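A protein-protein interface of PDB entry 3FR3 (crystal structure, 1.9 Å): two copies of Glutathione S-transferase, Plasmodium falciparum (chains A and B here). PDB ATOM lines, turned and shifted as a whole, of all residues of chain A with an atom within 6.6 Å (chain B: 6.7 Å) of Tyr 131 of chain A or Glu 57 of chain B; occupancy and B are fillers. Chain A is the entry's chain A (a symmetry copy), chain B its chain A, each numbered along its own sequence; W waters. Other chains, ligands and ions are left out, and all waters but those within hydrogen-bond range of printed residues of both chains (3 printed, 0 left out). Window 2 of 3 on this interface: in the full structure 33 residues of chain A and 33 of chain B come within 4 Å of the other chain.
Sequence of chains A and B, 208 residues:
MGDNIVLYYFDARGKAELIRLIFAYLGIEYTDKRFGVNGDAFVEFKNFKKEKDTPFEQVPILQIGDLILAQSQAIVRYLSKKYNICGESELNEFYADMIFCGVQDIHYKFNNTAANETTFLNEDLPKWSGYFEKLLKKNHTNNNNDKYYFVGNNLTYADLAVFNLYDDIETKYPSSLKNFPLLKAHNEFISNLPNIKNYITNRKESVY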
ATOM      1  N   ASP A 124      17.325 -10.285  18.275  1.00  0.00           N
ATOM      2  CA  ASP A 124      18.764 -10.554  18.193  1.00  0.00           C
ATOM      3  C   ASP A 124      19.578  -9.265  18.049  1.00  0.00           C
ATOM      4  O   ASP A 124      20.578  -9.073  18.742  1.00  0.00           O
ATOM      5  CB  ASP A 124      19.073 -11.450  16.994  1.00  0.00           C
ATOM      6  CG  ASP A 124      18.861 -12.928  17.289  1.00  0.00           C
ATOM      7  OD1 ASP A 124      18.383 -13.610  16.404  1.00  0.00           O
ATOM      8  OD2 ASP A 124      19.143 -13.410  18.404  1.00  0.00           O
ATOM      9  N   PRO A 126      18.900  -6.050  18.854  1.00  0.00           N
ATOM     10  CA  PRO A 126      19.005  -5.230  20.057  1.00  0.00           C
ATOM     11  C   PRO A 126      19.889  -5.868  21.111  1.00  0.00           C
ATOM     12  O   PRO A 126      20.667  -5.185  21.772  1.00  0.00           O
ATOM     13  CB  PRO A 126      17.538  -5.117  20.584  1.00  0.00           C
ATOM     14  CG  PRO A 126      16.668  -5.737  19.615  1.00  0.00           C
ATOM     15  CD  PRO A 126      17.497  -6.434  18.549  1.00  0.00           C
ATOM     16  N   LYS A 127      19.803  -7.187  21.234  1.00  0.00           N
ATOM     17  CA  LYS A 127      20.507  -7.893  22.267  1.00  0.00           C
ATOM     18  C   LYS A 127      22.002  -7.817  21.999  1.00  0.00           C
ATOM     19  O   LYS A 127      22.807  -7.537  22.898  1.00  0.00           O
ATOM     20  CB  LYS A 127      20.059  -9.352  22.183  1.00  0.00           C
ATOM     21  CG  LYS A 127      20.335 -10.194  23.340  1.00  0.00           C
ATOM     22  CD  LYS A 127      19.493 -11.452  23.182  1.00  0.00           C
ATOM     23  CE  LYS A 127      20.101 -12.457  22.226  1.00  0.00           C
ATOM     24  NZ  LYS A 127      19.261 -13.700  22.295  1.00  0.00           N
ATOM     25  N   TRP A 128      22.371  -8.074  20.750  1.00  0.00           N
ATOM     26  CA  TRP A 128      23.797  -7.993  20.356  1.00  0.00           C
ATOM     27  C   TRP A 128      24.340  -6.590  20.446  1.00  0.00           C
ATOM     28  O   TRP A 128      25.491  -6.397  20.853  1.00  0.00           O
ATOM     29  CB  TRP A 128      24.001  -8.622  18.967  1.00  0.00           C
ATOM     30  CG  TRP A 128      24.125 -10.107  19.146  1.00  0.00           C
ATOM     31  CD1 TRP A 128      23.121 -11.005  19.192  1.00  0.00           C
ATOM     32  CD2 TRP A 128      25.336 -10.846  19.345  1.00  0.00           C
ATOM     33  NE1 TRP A 128      23.604 -12.264  19.397  1.00  0.00           N
ATOM     34  CE2 TRP A 128      24.969 -12.203  19.506  1.00  0.00           C
ATOM     35  CE3 TRP A 128      26.679 -10.493  19.374  1.00  0.00           C
ATOM     36  CZ2 TRP A 128      25.904 -13.220  19.696  1.00  0.00           C
ATOM     37  CZ3 TRP A 128      27.625 -11.501  19.592  1.00  0.00           C
ATOM     38  CH2 TRP A 128      27.218 -12.861  19.757  1.00  0.00           C
ATOM     39  N   SER A 129      23.531  -5.611  20.041  1.00  0.00           N
ATOM     40  CA  SER A 129      23.860  -4.208  20.231  1.00  0.00           C
ATOM     41  C   SER A 129      24.132  -3.858  21.670  1.00  0.00           C
ATOM     42  O   SER A 129      25.142  -3.184  22.000  1.00  0.00           O
ATOM     43  CB  SER A 129      22.794  -3.276  19.618  1.00  0.00           C
ATOM     44  OG  SER A 129      22.649  -3.566  18.241  1.00  0.00           O
ATOM     45  N   GLY A 130      23.294  -4.373  22.565  1.00  0.00           N
ATOM     46  CA  GLY A 130      23.551  -4.214  23.992  1.00  0.00           C
ATOM     47  C   GLY A 130      24.833  -4.857  24.437  1.00  0.00           C
ATOM     48  O   GLY A 130      25.527  -4.306  25.270  1.00  0.00           O
ATOM     49  N   TYR A 131      25.203  -6.009  23.862  1.00  0.00           N
ATOM     50  CA  TYR A 131      26.505  -6.591  24.235  1.00  0.00           C
ATOM     51  C   TYR A 131      27.683  -5.661  23.912  1.00  0.00           C
ATOM     52  O   TYR A 131      28.636  -5.518  24.686  1.00  0.00           O
ATOM     53  CB  TYR A 131      26.756  -7.927  23.517  1.00  0.00           C
ATOM     54  CG  TYR A 131      25.686  -8.989  23.778  1.00  0.00           C
ATOM     55  CD1 TYR A 131      24.975  -9.036  25.007  1.00  0.00           C
ATOM     56  CD2 TYR A 131      25.411  -9.942  22.821  1.00  0.00           C
ATOM     57  CE1 TYR A 131      23.980 -10.038  25.225  1.00  0.00           C
ATOM     58  CE2 TYR A 131      24.438 -10.920  23.023  1.00  0.00           C
ATOM     59  CZ  TYR A 131      23.736 -10.960  24.244  1.00  0.00           C
ATOM     60  OH  TYR A 131      22.778 -11.927  24.418  1.00  0.00           O
ATOM     61  N   PHE A 132      27.645  -5.087  22.731  1.00  0.00           N
ATOM     62  CA  PHE A 132      28.737  -4.155  22.321  1.00  0.00           C
ATOM     63  C   PHE A 132      28.711  -2.883  23.098  1.00  0.00           C
ATOM     64  O   PHE A 132      29.772  -2.401  23.509  1.00  0.00           O
ATOM     65  CB  PHE A 132      28.755  -3.893  20.807  1.00  0.00           C
ATOM     66  CG  PHE A 132      28.955  -5.170  19.970  1.00  0.00           C
ATOM     67  CD1 PHE A 132      27.954  -5.639  19.121  1.00  0.00           C
ATOM     68  CD2 PHE A 132      30.168  -5.878  20.034  1.00  0.00           C
ATOM     69  CE1 PHE A 132      28.145  -6.845  18.348  1.00  0.00           C
ATOM     70  CE2 PHE A 132      30.358  -7.034  19.267  1.00  0.00           C
ATOM     71  CZ  PHE A 132      29.324  -7.519  18.430  1.00  0.00           C
ATOM     72  N   GLU A 133      27.511  -2.367  23.360  1.00  0.00           N
ATOM     73  CA  GLU A 133      27.337  -1.170  24.182  1.00  0.00           C
ATOM     74  C   GLU A 133      27.993  -1.386  25.533  1.00  0.00           C
ATOM     75  O   GLU A 133      28.700  -0.523  26.030  1.00  0.00           O
ATOM     76  CB  GLU A 133      25.827  -0.814  24.274  1.00  0.00           C
ATOM     77  CG  GLU A 133      25.424   0.520  25.005  1.00  0.00           C
ATOM     78  CD  GLU A 133      25.654   1.748  24.170  1.00  0.00           C
ATOM     79  OE1 GLU A 133      26.103   1.613  23.026  1.00  0.00           O
ATOM     80  OE2 GLU A 133      25.372   2.860  24.639  1.00  0.00           O
ATOM     81  N   LYS A 134      27.745  -2.531  26.166  1.00  0.00           N
ATOM     82  CA  LYS A 134      28.354  -2.871  27.436  1.00  0.00           C
ATOM     83  C   LYS A 134      29.879  -3.048  27.380  1.00  0.00           C
ATOM     84  O   LYS A 134      30.614  -2.631  28.308  1.00  0.00           O
ATOM     85  CB  LYS A 134      27.674  -4.113  28.001  1.00  0.00           C
ATOM     86  CG  LYS A 134      28.141  -4.530  29.349  1.00  0.00           C
ATOM     87  CD  LYS A 134      27.090  -5.499  29.932  1.00  0.00           C
ATOM     88  CE  LYS A 134      27.609  -6.908  29.965  1.00  0.00           C
ATOM     89  NZ  LYS A 134      28.595  -7.033  31.071  1.00  0.00           N
ATOM     90  N   LEU A 135      30.393  -3.654  26.301  1.00  0.00           N
ATOM     91  CA  LEU A 135      31.856  -3.755  26.128  1.00  0.00           C
ATOM     92  C   LEU A 135      32.534  -2.384  26.058  1.00  0.00           C
ATOM     93  O   LEU A 135      33.628  -2.164  26.601  1.00  0.00           O
ATOM     94  CB  LEU A 135      32.207  -4.608  24.897  1.00  0.00           C
ATOM     95  CG  LEU A 135      31.931  -6.098  25.172  1.00  0.00           C
ATOM     96  CD1 LEU A 135      31.921  -6.932  23.860  1.00  0.00           C
ATOM     97  CD2 LEU A 135      32.959  -6.685  26.135  1.00  0.00           C
ATOM     98  N   LEU A 136      31.895  -1.480  25.354  1.00  0.00           N
ATOM     99  CA  LEU A 136      32.411  -0.117  25.222  1.00  0.00           C
ATOM    100  C   LEU A 136      32.336   0.609  26.548  1.00  0.00           C
ATOM    101  O   LEU A 136      33.257   1.284  26.924  1.00  0.00           O
ATOM    102  CB  LEU A 136      31.562   0.627  24.237  1.00  0.00           C
ATOM    103  CG  LEU A 136      32.042   0.609  22.805  1.00  0.00           C
ATOM    104  CD1 LEU A 136      30.941   1.227  21.990  1.00  0.00           C
ATOM    105  CD2 LEU A 136      33.362   1.376  22.648  1.00  0.00           C
ATOM    106  N   PHE A 150      37.132  -0.099  21.657  1.00  0.00           N
ATOM    107  CA  PHE A 150      36.767  -1.300  22.363  1.00  0.00           C
ATOM    108  C   PHE A 150      37.833  -1.792  23.272  1.00  0.00           C
ATOM    109  O   PHE A 150      37.540  -2.256  24.366  1.00  0.00           O
ATOM    110  CB  PHE A 150      36.323  -2.389  21.386  1.00  0.00           C
ATOM    111  CG  PHE A 150      34.922  -2.221  20.960  1.00  0.00           C
ATOM    112  CD1 PHE A 150      34.631  -1.456  19.849  1.00  0.00           C
ATOM    113  CD2 PHE A 150      33.858  -2.741  21.743  1.00  0.00           C
ATOM    114  CE1 PHE A 150      33.334  -1.211  19.482  1.00  0.00           C
ATOM    115  CE2 PHE A 150      32.493  -2.554  21.341  1.00  0.00           C
ATOM    116  CZ  PHE A 150      32.247  -1.781  20.212  1.00  0.00           C
ATOM    117  N   PHE A 180      21.560   3.104  21.500  1.00  0.00           N
ATOM    118  CA  PHE A 180      22.887   2.679  21.959  1.00  0.00           C
ATOM    119  C   PHE A 180      23.882   3.804  21.720  1.00  0.00           C
ATOM    120  O   PHE A 180      24.576   3.801  20.702  1.00  0.00           O
ATOM    121  CB  PHE A 180      23.309   1.432  21.170  1.00  0.00           C
ATOM    122  CG  PHE A 180      22.341   0.292  21.343  1.00  0.00           C
ATOM    123  CD1 PHE A 180      21.307   0.091  20.438  1.00  0.00           C
ATOM    124  CD2 PHE A 180      22.434  -0.522  22.440  1.00  0.00           C
ATOM    125  CE1 PHE A 180      20.378  -0.939  20.634  1.00  0.00           C
ATOM    126  CE2 PHE A 180      21.503  -1.552  22.626  1.00  0.00           C
ATOM    127  CZ  PHE A 180      20.474  -1.720  21.725  1.00  0.00           C
ATOM    128  N   PHE B  45      21.935 -23.361  32.209  1.00  0.00           N
ATOM    129  CA  PHE B  45      22.584 -22.293  31.440  1.00  0.00           C
ATOM    130  C   PHE B  45      22.028 -20.925  31.810  1.00  0.00           C
ATOM    131  O   PHE B  45      22.770 -19.993  32.070  1.00  0.00           O
ATOM    132  CB  PHE B  45      22.357 -22.536  29.968  1.00  0.00           C
ATOM    133  CG  PHE B  45      22.991 -21.489  29.086  1.00  0.00           C
ATOM    134  CD1 PHE B  45      22.269 -20.895  28.055  1.00  0.00           C
ATOM    135  CD2 PHE B  45      24.318 -21.086  29.308  1.00  0.00           C
ATOM    136  CE1 PHE B  45      22.900 -19.935  27.221  1.00  0.00           C
ATOM    137  CE2 PHE B  45      24.923 -20.120  28.469  1.00  0.00           C
ATOM    138  CZ  PHE B  45      24.201 -19.573  27.446  1.00  0.00           C
ATOM    139  N   LYS B  49      24.103 -17.802  33.428  1.00  0.00           N
ATOM    140  CA  LYS B  49      24.238 -16.441  32.910  1.00  0.00           C
ATOM    141  C   LYS B  49      23.907 -15.420  33.987  1.00  0.00           C
ATOM    142  O   LYS B  49      24.474 -14.323  33.994  1.00  0.00           O
ATOM    143  CB  LYS B  49      23.360 -16.209  31.697  1.00  0.00           C
ATOM    144  CG  LYS B  49      23.796 -16.896  30.433  1.00  0.00           C
ATOM    145  CD  LYS B  49      22.836 -16.584  29.299  1.00  0.00           C
ATOM    146  CE  LYS B  49      21.533 -17.364  29.326  1.00  0.00           C
ATOM    147  NZ  LYS B  49      20.540 -16.852  28.287  1.00  0.00           N
ATOM    148  N   THR B  54      28.884 -12.758  31.334  1.00  0.00           N
ATOM    149  CA  THR B  54      29.422 -13.203  30.027  1.00  0.00           C
ATOM    150  C   THR B  54      29.282 -12.079  28.964  1.00  0.00           C
ATOM    151  O   THR B  54      28.343 -11.273  29.019  1.00  0.00           O
ATOM    152  CB  THR B  54      28.772 -14.480  29.551  1.00  0.00           C
ATOM    153  OG1 THR B  54      27.398 -14.205  29.209  1.00  0.00           O
ATOM    154  CG2 THR B  54      28.849 -15.526  30.661  1.00  0.00           C
ATOM    155  N   PRO B  55      30.266 -11.965  28.048  1.00  0.00           N
ATOM    156  CA  PRO B  55      30.099 -10.870  27.143  1.00  0.00           C
ATOM    157  C   PRO B  55      28.944 -10.994  26.168  1.00  0.00           C
ATOM    158  O   PRO B  55      28.384  -9.961  25.787  1.00  0.00           O
ATOM    159  CB  PRO B  55      31.445 -10.790  26.404  1.00  0.00           C
ATOM    160  CG  PRO B  55      32.007 -12.123  26.524  1.00  0.00           C
ATOM    161  CD  PRO B  55      31.576 -12.613  27.906  1.00  0.00           C
ATOM    162  N   PHE B  56      28.613 -12.209  25.743  1.00  0.00           N
ATOM    163  CA  PHE B  56      27.613 -12.393  24.679  1.00  0.00           C
ATOM    164  C   PHE B  56      26.558 -13.402  25.064  1.00  0.00           C
ATOM    165  O   PHE B  56      25.826 -13.854  24.175  1.00  0.00           O
ATOM    166  CB  PHE B  56      28.276 -12.879  23.392  1.00  0.00           C
ATOM    167  CG  PHE B  56      29.381 -11.940  22.905  1.00  0.00           C
ATOM    168  CD1 PHE B  56      30.713 -12.365  22.911  1.00  0.00           C
ATOM    169  CD2 PHE B  56      29.086 -10.627  22.530  1.00  0.00           C
ATOM    170  CE1 PHE B  56      31.769 -11.514  22.446  1.00  0.00           C
ATOM    171  CE2 PHE B  56      30.143  -9.752  22.052  1.00  0.00           C
ATOM    172  CZ  PHE B  56      31.473 -10.203  22.021  1.00  0.00           C
ATOM    173  N   GLU B  57      26.478 -13.761  26.357  1.00  0.00           N
ATOM    174  CA  GLU B  57      25.487 -14.798  26.814  1.00  0.00           C
ATOM    175  C   GLU B  57      25.556 -16.104  26.037  1.00  0.00           C
ATOM    176  O   GLU B  57      24.533 -16.756  25.758  1.00  0.00           O
ATOM    177  CB  GLU B  57      24.052 -14.241  26.826  1.00  0.00           C
ATOM    178  CG  GLU B  57      23.954 -12.985  27.764  1.00  0.00           C
ATOM    179  CD  GLU B  57      22.530 -12.424  27.857  1.00  0.00           C
ATOM    180  OE1 GLU B  57      22.052 -12.271  28.988  1.00  0.00           O
ATOM    181  OE2 GLU B  57      21.917 -12.133  26.814  1.00  0.00           O
ATOM    182  N   GLN B  58      26.788 -16.502  25.706  1.00  0.00           N
ATOM    183  CA  GLN B  58      27.072 -17.748  25.052  1.00  0.00           C
ATOM    184  C   GLN B  58      28.180 -18.499  25.779  1.00  0.00           C
ATOM    185  O   GLN B  58      28.953 -17.927  26.516  1.00  0.00           O
ATOM    186  CB  GLN B  58      27.600 -17.571  23.601  1.00  0.00           C
ATOM    187  CG  GLN B  58      26.717 -16.674  22.727  1.00  0.00           C
ATOM    188  CD  GLN B  58      27.426 -16.351  21.390  1.00  0.00           C
ATOM    189  OE1 GLN B  58      26.833 -16.557  20.321  1.00  0.00           O
ATOM    190  NE2 GLN B  58      28.705 -15.961  21.448  1.00  0.00           N
ATOM    191  N   VAL B  59      28.193 -19.804  25.529  1.00  0.00           N
ATOM    192  CA  VAL B  59      29.300 -20.633  25.901  1.00  0.00           C
ATOM    193  C   VAL B  59      29.919 -21.202  24.608  1.00  0.00           C
ATOM    194  O   VAL B  59      29.278 -21.238  23.586  1.00  0.00           O
ATOM    195  CB  VAL B  59      28.810 -21.762  26.844  1.00  0.00           C
ATOM    196  CG1 VAL B  59      28.542 -21.146  28.283  1.00  0.00           C
ATOM    197  CG2 VAL B  59      27.621 -22.558  26.221  1.00  0.00           C
ATOM    198  N   ILE B  61      32.610 -20.688  27.815  1.00  0.00           N
ATOM    199  CA  ILE B  61      33.282 -19.663  28.607  1.00  0.00           C
ATOM    200  C   ILE B  61      34.420 -20.368  29.327  1.00  0.00           C
ATOM    201  O   ILE B  61      34.228 -21.456  29.846  1.00  0.00           O
ATOM    202  CB  ILE B  61      32.353 -19.051  29.726  1.00  0.00           C
ATOM    203  CG1 ILE B  61      31.250 -18.186  29.098  1.00  0.00           C
ATOM    204  CG2 ILE B  61      33.228 -18.330  30.779  1.00  0.00           C
ATOM    205  CD1 ILE B  61      31.764 -16.937  28.416  1.00  0.00           C
HETATM  206  O   HOH W   1      20.666 -14.616  24.893  1.00  0.00           O
HETATM  207  O   HOH W   2      23.390 -14.463  22.930  1.00  0.00           O
HETATM  208  O   HOH W   3      28.867  -7.368  26.717  1.00  0.00           O
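OH of Tyr 131 of chain A is in hydrogen-bond range of OE2 of Glu 57 of chain B (2.6 Å).
The backbone NH (N) of Glu 57 of chain B lies within hydrogen-bond range of the side-chain hydroxyl (OG1) of Thr 54 of chain B.
Among the printed residues, merely in contact across the chains: Trp 128 of chain A with Phe 56 of chain B (3.4 Å), Trp 128 of chain A with Gln 58 of chain B (3.5 Å), Tyr 131 of chain A with Pro 55 of chain B (3.5 Å), Tyr 131 of chain A with Phe 56 of chain B (3.4 Å), Phe 132 of chain A with Phe 56 of chain B (3.9 Å) and Leu 135 of chain A with Phe 56 of chain B (3.8 Å).
Lys 127 of chain A touches none of the printed residues of chain B.
Ser 129 of chain A touches none of the printed residues of chain B.
Of chain B, only Pro 55 (3.5 Å), Phe 56 (3.4 Å) and Glu 57 (2.6 Å) come within 4 Å of Tyr 131 of chain A.
Of the printed residues of chain B, Phe 132 of chain A touches Phe 56.
Printed residues of chain A within 4 Å of Pro 55 of chain B: Tyr 131.
Glu 57 of chain B touches just one residue of chain A: Tyr 131.
The nearest residue of chain A that does not touch Glu 57 of chain B is Lys 127 of chain A (4.3 Å).
The nearest printed residue of chain A that does not touch Pro 55 of chain B is Leu 135 of chain A (4.4 Å).
Of the 9 printed residues of chain B, 4 touch a printed residue of chain A.
Hydrophobic or aromatic side chains of chain B within 4 Å of the printed part of chain A: Phe 56.
Among the printed residues, 7 pairs touch across the chains.
Among the printed residues, no Asp or Glu carboxylate lies within 4 Å of a Lys or Arg side-chain nitrogen of the other chain.
No position is printed for both chains.
Of the 7 pairs that touch across the chains among the printed residues, none has its exchanged pair printed and touching as well.
Water W3 lies within hydrogen-bond range of the backbone carbonyl oxygen of Tyr 131 of chain A and the backbone carbonyl oxygen of Pro 55 of chain B.
Water W2 bridges the backbone carbonyl oxygen of Phe 56 of chain B (2.8 Å) and the side-chain hydroxyl of Tyr 131 of chain A (3.0 Å).
Water W1 lies within hydrogen-bond range of NZ of Lys 127 of chain A (3.1 Å), OE2 of Glu 57 of chain B (3.4 Å) and OH of Tyr 131 of chain A (3.5 Å).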
